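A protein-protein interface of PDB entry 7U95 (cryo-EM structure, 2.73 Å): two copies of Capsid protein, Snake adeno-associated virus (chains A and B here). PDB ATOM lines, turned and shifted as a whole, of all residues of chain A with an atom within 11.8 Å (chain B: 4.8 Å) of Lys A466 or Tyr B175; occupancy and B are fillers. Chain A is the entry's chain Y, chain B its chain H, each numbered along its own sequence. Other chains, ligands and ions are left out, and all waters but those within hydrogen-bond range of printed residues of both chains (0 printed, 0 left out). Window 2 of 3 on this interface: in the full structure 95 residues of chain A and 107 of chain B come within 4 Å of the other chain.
SG of Cys B172 is in hydrogen-bond range of OE1 of Glu B174 (3.2 Å). OG of Ser A205 lies close to N of His A512. The guanidinium group (NE) of Arg A467 sits at hydrogen-bond distance from the side-chain amide oxygen (OD1) of Asn A469. The guanidinium group (NH2) of Arg A467 is in hydrogen-bond range of the backbone carbonyl oxygen (O) of Pro A470, at 3.4 Å. NH1 of Arg A467 is in salt-bridge range of OE2 of Glu A471, 3.9 Å away.
Along chain B the printed residues that touch a printed residue of chain A span positions 126 to 176. Among the printed residues, no Asp or Glu carboxylate lies within 4 Å of a Lys or Arg side-chain nitrogen of the other chain.
Of chain B, only Asp B126, Tyr B171, Tyr B175 and Phe B176 come within 4 Å of Lys A466. Of the printed residues of chain B, Arg A467 touches Tyr B171 (3.6 Å). Printed residues of chain B within 4 Å of Trp A468: Cys B172 (3.7 Å). Printed residues of chain B within 4 Å of His A512: Asp B126 and Tyr B171. Asp B126 touches just these residues of chain A: Lys A466 and His A512. Of chain A, only Trp A468 (3.7 Å) comes within 4 Å of Cys B172. No residue of chain A comes within 4 Å of Glu B174. Of the printed residues of chain A, Tyr B175 touches Lys A466 (3.1 Å). Pro B177 touches none of the printed residues of chain A. The nearest printed residue of chain B that does not touch Lys A466 is Cys B172 (4.8 Å).
NZ of Lys A466 lies close to O of Tyr B175 (3.2 Å).
Among the printed residues, merely in contact across the chains: Lys A466 with Asp B126, Lys A466 with Tyr B171, Lys A466 with Phe B176, Arg A467 with Tyr B171, Trp A468 with Cys B172, His A512 with Asp B126 and His A512 with Tyr B171.
No position is printed for both chains. Of the 8 pairs that touch across the chains among the printed residues, none has its exchanged pair printed and touching as well.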
ATOM      1  N   ASN A  79      13.070 -26.814  -0.206  1.00  0.00           N
ATOM      2  CA  ASN A  79      13.817 -25.748  -0.852  1.00  0.00           C
ATOM      3  C   ASN A  79      14.309 -24.648   0.074  1.00  0.00           C
ATOM      4  O   ASN A  79      15.358 -24.069  -0.199  1.00  0.00           O
ATOM      5  CB  ASN A  79      12.966 -25.142  -1.955  1.00  0.00           C
ATOM      6  CG  ASN A  79      12.684 -26.131  -3.031  1.00  0.00           C
ATOM      7  OD1 ASN A  79      11.546 -26.316  -3.448  1.00  0.00           O
ATOM      8  ND2 ASN A  79      13.730 -26.809  -3.477  1.00  0.00           N
ATOM      9  N   THR A  81      15.233 -22.634   3.810  1.00  0.00           N
ATOM     10  CA  THR A  81      15.770 -22.841   5.148  1.00  0.00           C
ATOM     11  C   THR A  81      15.178 -21.924   6.206  1.00  0.00           C
ATOM     12  O   THR A  81      15.636 -21.961   7.348  1.00  0.00           O
ATOM     13  CB  THR A  81      17.288 -22.677   5.151  1.00  0.00           C
ATOM     14  OG1 THR A  81      17.629 -21.373   4.675  1.00  0.00           O
ATOM     15  CG2 THR A  81      17.937 -23.719   4.280  1.00  0.00           C
ATOM     16  N   SER A 205      24.368 -30.428  10.853  1.00  0.00           N
ATOM     17  CA  SER A 205      25.213 -31.555  10.492  1.00  0.00           C
ATOM     18  C   SER A 205      26.491 -31.651  11.312  1.00  0.00           C
ATOM     19  O   SER A 205      27.319 -32.520  11.031  1.00  0.00           O
ATOM     20  CB  SER A 205      25.564 -31.487   9.011  1.00  0.00           C
ATOM     21  OG  SER A 205      26.315 -30.326   8.732  1.00  0.00           O
ATOM     22  N   LYS A 462      15.867 -18.748   0.657  1.00  0.00           N
ATOM     23  CA  LYS A 462      16.441 -19.750  -0.216  1.00  0.00           C
ATOM     24  C   LYS A 462      17.954 -19.714  -0.058  1.00  0.00           C
ATOM     25  O   LYS A 462      18.547 -18.655   0.151  1.00  0.00           O
ATOM     26  CB  LYS A 462      16.030 -19.492  -1.664  1.00  0.00           C
ATOM     27  CG  LYS A 462      16.376 -20.601  -2.628  1.00  0.00           C
ATOM     28  CD  LYS A 462      16.003 -20.205  -4.044  1.00  0.00           C
ATOM     29  CE  LYS A 462      14.497 -20.085  -4.198  1.00  0.00           C
ATOM     30  NZ  LYS A 462      14.104 -19.666  -5.571  1.00  0.00           N
ATOM     31  N   GLU A 463      18.577 -20.883  -0.147  1.00  0.00           N
ATOM     32  CA  GLU A 463      19.946 -21.073   0.308  1.00  0.00           C
ATOM     33  C   GLU A 463      20.794 -21.655  -0.810  1.00  0.00           C
ATOM     34  O   GLU A 463      20.288 -22.100  -1.841  1.00  0.00           O
ATOM     35  CB  GLU A 463      20.000 -22.024   1.501  1.00  0.00           C
ATOM     36  CG  GLU A 463      19.866 -23.472   1.074  1.00  0.00           C
ATOM     37  CD  GLU A 463      18.477 -23.817   0.604  1.00  0.00           C
ATOM     38  OE1 GLU A 463      17.614 -22.920   0.582  1.00  0.00           O
ATOM     39  OE2 GLU A 463      18.250 -24.981   0.227  1.00  0.00           O
ATOM     40  N   SER A 464      22.104 -21.641  -0.592  1.00  0.00           N
ATOM     41  CA  SER A 464      23.049 -22.334  -1.460  1.00  0.00           C
ATOM     42  C   SER A 464      23.906 -23.238  -0.588  1.00  0.00           C
ATOM     43  O   SER A 464      24.698 -22.753   0.225  1.00  0.00           O
ATOM     44  CB  SER A 464      23.913 -21.346  -2.238  1.00  0.00           C
ATOM     45  OG  SER A 464      24.722 -20.586  -1.359  1.00  0.00           O
ATOM     46  N   SER A 465      23.751 -24.546  -0.761  1.00  0.00           N
ATOM     47  CA  SER A 465      24.544 -25.535  -0.048  1.00  0.00           C
ATOM     48  C   SER A 465      25.658 -25.993  -0.973  1.00  0.00           C
ATOM     49  O   SER A 465      25.395 -26.371  -2.117  1.00  0.00           O
ATOM     50  CB  SER A 465      23.686 -26.727   0.369  1.00  0.00           C
ATOM     51  OG  SER A 465      22.653 -26.331   1.246  1.00  0.00           O
ATOM     52  N   LYS A 466      26.897 -25.931  -0.499  1.00  0.00           N
ATOM     53  CA  LYS A 466      28.016 -26.415  -1.286  1.00  0.00           C
ATOM     54  C   LYS A 466      28.457 -27.823  -0.915  1.00  0.00           C
ATOM     55  O   LYS A 466      29.502 -28.269  -1.390  1.00  0.00           O
ATOM     56  CB  LYS A 466      29.188 -25.447  -1.219  1.00  0.00           C
ATOM     57  CG  LYS A 466      28.877 -24.159  -1.956  1.00  0.00           C
ATOM     58  CD  LYS A 466      30.103 -23.304  -2.158  1.00  0.00           C
ATOM     59  CE  LYS A 466      30.984 -23.898  -3.238  1.00  0.00           C
ATOM     60  NZ  LYS A 466      30.341 -23.831  -4.580  1.00  0.00           N
ATOM     61  N   ARG A 467      27.721 -28.522  -0.057  1.00  0.00           N
ATOM     62  CA  ARG A 467      28.017 -29.933   0.128  1.00  0.00           C
ATOM     63  C   ARG A 467      27.858 -30.668  -1.191  1.00  0.00           C
ATOM     64  O   ARG A 467      27.032 -30.310  -2.032  1.00  0.00           O
ATOM     65  CB  ARG A 467      27.114 -30.553   1.186  1.00  0.00           C
ATOM     66  CG  ARG A 467      25.658 -30.532   0.841  1.00  0.00           C
ATOM     67  CD  ARG A 467      24.838 -31.110   1.964  1.00  0.00           C
ATOM     68  NE  ARG A 467      24.994 -32.547   2.119  1.00  0.00           N
ATOM     69  CZ  ARG A 467      24.505 -33.229   3.146  1.00  0.00           C
ATOM     70  NH1 ARG A 467      23.868 -32.596   4.109  1.00  0.00           N
ATOM     71  NH2 ARG A 467      24.668 -34.536   3.223  1.00  0.00           N
ATOM     72  N   TRP A 468      28.685 -31.690  -1.385  1.00  0.00           N
ATOM     73  CA  TRP A 468      28.688 -32.420  -2.644  1.00  0.00           C
ATOM     74  C   TRP A 468      27.536 -33.412  -2.710  1.00  0.00           C
ATOM     75  O   TRP A 468      26.792 -33.450  -3.691  1.00  0.00           O
ATOM     76  CB  TRP A 468      30.024 -33.137  -2.806  1.00  0.00           C
ATOM     77  CG  TRP A 468      30.197 -33.845  -4.090  1.00  0.00           C
ATOM     78  CD1 TRP A 468      30.069 -35.176  -4.313  1.00  0.00           C
ATOM     79  CD2 TRP A 468      30.574 -33.263  -5.334  1.00  0.00           C
ATOM     80  NE1 TRP A 468      30.322 -35.459  -5.628  1.00  0.00           N
ATOM     81  CE2 TRP A 468      30.637 -34.296  -6.274  1.00  0.00           C
ATOM     82  CE3 TRP A 468      30.854 -31.962  -5.746  1.00  0.00           C
ATOM     83  CZ2 TRP A 468      30.968 -34.072  -7.595  1.00  0.00           C
ATOM     84  CZ3 TRP A 468      31.181 -31.745  -7.054  1.00  0.00           C
ATOM     85  CH2 TRP A 468      31.235 -32.790  -7.964  1.00  0.00           C
ATOM     86  N   ASN A 469      27.364 -34.200  -1.666  1.00  0.00           N
ATOM     87  CA  ASN A 469      26.415 -35.293  -1.655  1.00  0.00           C
ATOM     88  C   ASN A 469      24.992 -34.793  -1.450  1.00  0.00           C
ATOM     89  O   ASN A 469      24.774 -33.700  -0.931  1.00  0.00           O
ATOM     90  CB  ASN A 469      26.792 -36.266  -0.552  1.00  0.00           C
ATOM     91  CG  ASN A 469      26.896 -35.597   0.776  1.00  0.00           C
ATOM     92  OD1 ASN A 469      27.032 -34.388   0.847  1.00  0.00           O
ATOM     93  ND2 ASN A 469      26.805 -36.366   1.839  1.00  0.00           N
ATOM     94  N   PRO A 470      23.999 -35.577  -1.853  1.00  0.00           N
ATOM     95  CA  PRO A 470      22.607 -35.153  -1.702  1.00  0.00           C
ATOM     96  C   PRO A 470      22.168 -35.109  -0.246  1.00  0.00           C
ATOM     97  O   PRO A 470      22.815 -35.640   0.652  1.00  0.00           O
ATOM     98  CB  PRO A 470      21.843 -36.212  -2.495  1.00  0.00           C
ATOM     99  CG  PRO A 470      22.715 -37.368  -2.508  1.00  0.00           C
ATOM    100  CD  PRO A 470      24.092 -36.832  -2.610  1.00  0.00           C
ATOM    101  N   GLU A 471      21.026 -34.460  -0.030  1.00  0.00           N
ATOM    102  CA  GLU A 471      20.443 -34.248   1.283  1.00  0.00           C
ATOM    103  C   GLU A 471      19.146 -35.021   1.441  1.00  0.00           C
ATOM    104  O   GLU A 471      18.477 -35.358   0.465  1.00  0.00           O
ATOM    105  CB  GLU A 471      20.162 -32.767   1.529  1.00  0.00           C
ATOM    106  CG  GLU A 471      21.389 -31.943   1.743  1.00  0.00           C
ATOM    107  CD  GLU A 471      21.075 -30.489   1.901  1.00  0.00           C
ATOM    108  OE1 GLU A 471      19.931 -30.110   1.605  1.00  0.00           O
ATOM    109  OE2 GLU A 471      21.962 -29.724   2.327  1.00  0.00           O
ATOM    110  N   ILE A 509      17.006 -29.793   5.750  1.00  0.00           N
ATOM    111  CA  ILE A 509      18.253 -29.436   5.091  1.00  0.00           C
ATOM    112  C   ILE A 509      19.337 -29.329   6.139  1.00  0.00           C
ATOM    113  O   ILE A 509      19.173 -28.629   7.142  1.00  0.00           O
ATOM    114  CB  ILE A 509      18.136 -28.130   4.294  1.00  0.00           C
ATOM    115  CG1 ILE A 509      17.293 -28.343   3.050  1.00  0.00           C
ATOM    116  CG2 ILE A 509      19.492 -27.627   3.906  1.00  0.00           C
ATOM    117  CD1 ILE A 509      17.041 -27.089   2.306  1.00  0.00           C
ATOM    118  N   SER A 510      20.438 -30.029   5.917  1.00  0.00           N
ATOM    119  CA  SER A 510      21.547 -29.979   6.845  1.00  0.00           C
ATOM    120  C   SER A 510      22.386 -28.746   6.580  1.00  0.00           C
ATOM    121  O   SER A 510      22.526 -28.304   5.439  1.00  0.00           O
ATOM    122  CB  SER A 510      22.402 -31.227   6.717  1.00  0.00           C
ATOM    123  OG  SER A 510      21.642 -32.365   7.043  1.00  0.00           O
ATOM    124  N   LYS A 511      22.929 -28.182   7.647  1.00  0.00           N
ATOM    125  CA  LYS A 511      23.858 -27.074   7.550  1.00  0.00           C
ATOM    126  C   LYS A 511      24.860 -27.220   8.680  1.00  0.00           C
ATOM    127  O   LYS A 511      24.489 -27.600   9.790  1.00  0.00           O
ATOM    128  CB  LYS A 511      23.112 -25.746   7.623  1.00  0.00           C
ATOM    129  CG  LYS A 511      23.964 -24.537   7.387  1.00  0.00           C
ATOM    130  CD  LYS A 511      23.151 -23.276   7.562  1.00  0.00           C
ATOM    131  CE  LYS A 511      22.114 -23.147   6.477  1.00  0.00           C
ATOM    132  NZ  LYS A 511      21.345 -21.897   6.629  1.00  0.00           N
ATOM    133  N   HIS A 512      26.129 -26.952   8.402  1.00  0.00           N
ATOM    134  CA  HIS A 512      27.134 -27.141   9.435  1.00  0.00           C
ATOM    135  C   HIS A 512      26.945 -26.124  10.549  1.00  0.00           C
ATOM    136  O   HIS A 512      26.544 -24.982  10.322  1.00  0.00           O
ATOM    137  CB  HIS A 512      28.546 -27.041   8.866  1.00  0.00           C
ATOM    138  CG  HIS A 512      28.851 -25.727   8.231  1.00  0.00           C
ATOM    139  ND1 HIS A 512      28.448 -25.409   6.956  1.00  0.00           N
ATOM    140  CD2 HIS A 512      29.505 -24.642   8.702  1.00  0.00           C
ATOM    141  CE1 HIS A 512      28.851 -24.187   6.663  1.00  0.00           C
ATOM    142  NE2 HIS A 512      29.493 -23.699   7.706  1.00  0.00           N
ATOM    143  N   ASP B 126      30.864 -21.413   3.790  1.00  0.00           N
ATOM    144  CA  ASP B 126      30.256 -22.642   3.296  1.00  0.00           C
ATOM    145  C   ASP B 126      30.950 -23.892   3.816  1.00  0.00           C
ATOM    146  O   ASP B 126      30.303 -24.929   3.973  1.00  0.00           O
ATOM    147  CB  ASP B 126      30.251 -22.631   1.771  1.00  0.00           C
ATOM    148  CG  ASP B 126      29.232 -21.670   1.209  1.00  0.00           C
ATOM    149  OD1 ASP B 126      28.277 -21.332   1.934  1.00  0.00           O
ATOM    150  OD2 ASP B 126      29.391 -21.228   0.055  1.00  0.00           O
ATOM    151  N   TYR B 171      32.307 -32.278   1.335  1.00  0.00           N
ATOM    152  CA  TYR B 171      32.548 -31.034   0.624  1.00  0.00           C
ATOM    153  C   TYR B 171      33.700 -31.227  -0.347  1.00  0.00           C
ATOM    154  O   TYR B 171      34.796 -31.618   0.059  1.00  0.00           O
ATOM    155  CB  TYR B 171      32.867 -29.907   1.600  1.00  0.00           C
ATOM    156  CG  TYR B 171      31.752 -29.597   2.554  1.00  0.00           C
ATOM    157  CD1 TYR B 171      30.744 -28.726   2.204  1.00  0.00           C
ATOM    158  CD2 TYR B 171      31.718 -30.165   3.808  1.00  0.00           C
ATOM    159  CE1 TYR B 171      29.731 -28.442   3.071  1.00  0.00           C
ATOM    160  CE2 TYR B 171      30.708 -29.885   4.679  1.00  0.00           C
ATOM    161  CZ  TYR B 171      29.718 -29.024   4.306  1.00  0.00           C
ATOM    162  OH  TYR B 171      28.700 -28.737   5.177  1.00  0.00           O
ATOM    163  N   CYS B 172      33.452 -30.956  -1.620  1.00  0.00           N
ATOM    164  CA  CYS B 172      34.508 -30.896  -2.618  1.00  0.00           C
ATOM    165  C   CYS B 172      35.017 -29.465  -2.682  1.00  0.00           C
ATOM    166  O   CYS B 172      34.246 -28.542  -2.956  1.00  0.00           O
ATOM    167  CB  CYS B 172      34.003 -31.350  -3.983  1.00  0.00           C
ATOM    168  SG  CYS B 172      35.242 -31.332  -5.277  1.00  0.00           S
ATOM    169  N   LEU B 173      36.299 -29.277  -2.419  1.00  0.00           N
ATOM    170  CA  LEU B 173      36.844 -27.935  -2.335  1.00  0.00           C
ATOM    171  C   LEU B 173      37.357 -27.417  -3.666  1.00  0.00           C
ATOM    172  O   LEU B 173      37.759 -26.255  -3.745  1.00  0.00           O
ATOM    173  CB  LEU B 173      37.958 -27.885  -1.291  1.00  0.00           C
ATOM    174  CG  LEU B 173      37.517 -27.684   0.158  1.00  0.00           C
ATOM    175  CD1 LEU B 173      36.719 -28.854   0.680  1.00  0.00           C
ATOM    176  CD2 LEU B 173      38.713 -27.473   1.014  1.00  0.00           C
ATOM    177  N   GLU B 174      37.295 -28.242  -4.701  1.00  0.00           N
ATOM    178  CA  GLU B 174      37.684 -27.802  -6.029  1.00  0.00           C
ATOM    179  C   GLU B 174      36.461 -27.229  -6.701  1.00  0.00           C
ATOM    180  O   GLU B 174      36.515 -26.821  -7.856  1.00  0.00           O
ATOM    181  CB  GLU B 174      38.241 -28.964  -6.845  1.00  0.00           C
ATOM    182  CG  GLU B 174      39.584 -29.484  -6.356  1.00  0.00           C
ATOM    183  CD  GLU B 174      39.471 -30.329  -5.104  1.00  0.00           C
ATOM    184  OE1 GLU B 174      38.358 -30.798  -4.797  1.00  0.00           O
ATOM    185  OE2 GLU B 174      40.502 -30.535  -4.431  1.00  0.00           O
ATOM    186  N   TYR B 175      35.349 -27.195  -5.978  1.00  0.00           N
ATOM    187  CA  TYR B 175      34.113 -26.660  -6.520  1.00  0.00           C
ATOM    188  C   TYR B 175      33.976 -25.207  -6.120  1.00  0.00           C
ATOM    189  O   TYR B 175      32.907 -24.618  -6.254  1.00  0.00           O
ATOM    190  CB  TYR B 175      32.931 -27.475  -6.010  1.00  0.00           C
ATOM    191  CG  TYR B 175      31.631 -27.166  -6.705  1.00  0.00           C
ATOM    192  CD1 TYR B 175      31.460 -27.441  -8.052  1.00  0.00           C
ATOM    193  CD2 TYR B 175      30.568 -26.605  -6.011  1.00  0.00           C
ATOM    194  CE1 TYR B 175      30.272 -27.161  -8.692  1.00  0.00           C
ATOM    195  CE2 TYR B 175      29.375 -26.320  -6.642  1.00  0.00           C
ATOM    196  CZ  TYR B 175      29.234 -26.601  -7.981  1.00  0.00           C
ATOM    197  OH  TYR B 175      28.049 -26.320  -8.615  1.00  0.00           O
ATOM    198  N   PHE B 176      35.054 -24.624  -5.616  1.00  0.00           N
ATOM    199  CA  PHE B 176      35.039 -23.229  -5.216  1.00  0.00           C
ATOM    200  C   PHE B 176      35.931 -22.444  -6.151  1.00  0.00           C
ATOM    201  O   PHE B 176      37.086 -22.808  -6.357  1.00  0.00           O
ATOM    202  CB  PHE B 176      35.565 -23.072  -3.797  1.00  0.00           C
ATOM    203  CG  PHE B 176      34.736 -23.753  -2.751  1.00  0.00           C
ATOM    204  CD1 PHE B 176      34.025 -23.009  -1.828  1.00  0.00           C
ATOM    205  CD2 PHE B 176      34.680 -25.134  -2.678  1.00  0.00           C
ATOM    206  CE1 PHE B 176      33.266 -23.627  -0.855  1.00  0.00           C
ATOM    207  CE2 PHE B 176      33.922 -25.760  -1.709  1.00  0.00           C
ATOM    208  CZ  PHE B 176      33.212 -25.006  -0.797  1.00  0.00           C
ATOM    209  N   PRO B 177      35.407 -21.359  -6.728  1.00  0.00           N
ATOM    210  CA  PRO B 177      36.257 -20.519  -7.569  1.00  0.00           C
ATOM    211  C   PRO B 177      37.541 -20.154  -6.837  1.00  0.00           C
ATOM    212  O   PRO B 177      37.468 -19.691  -5.703  1.00  0.00           O
ATOM    213  CB  PRO B 177      35.394 -19.284  -7.791  1.00  0.00           C
ATOM    214  CG  PRO B 177      33.994 -19.793  -7.710  1.00  0.00           C
ATOM    215  CD  PRO B 177      34.017 -20.879  -6.673  1.00  0.00           C
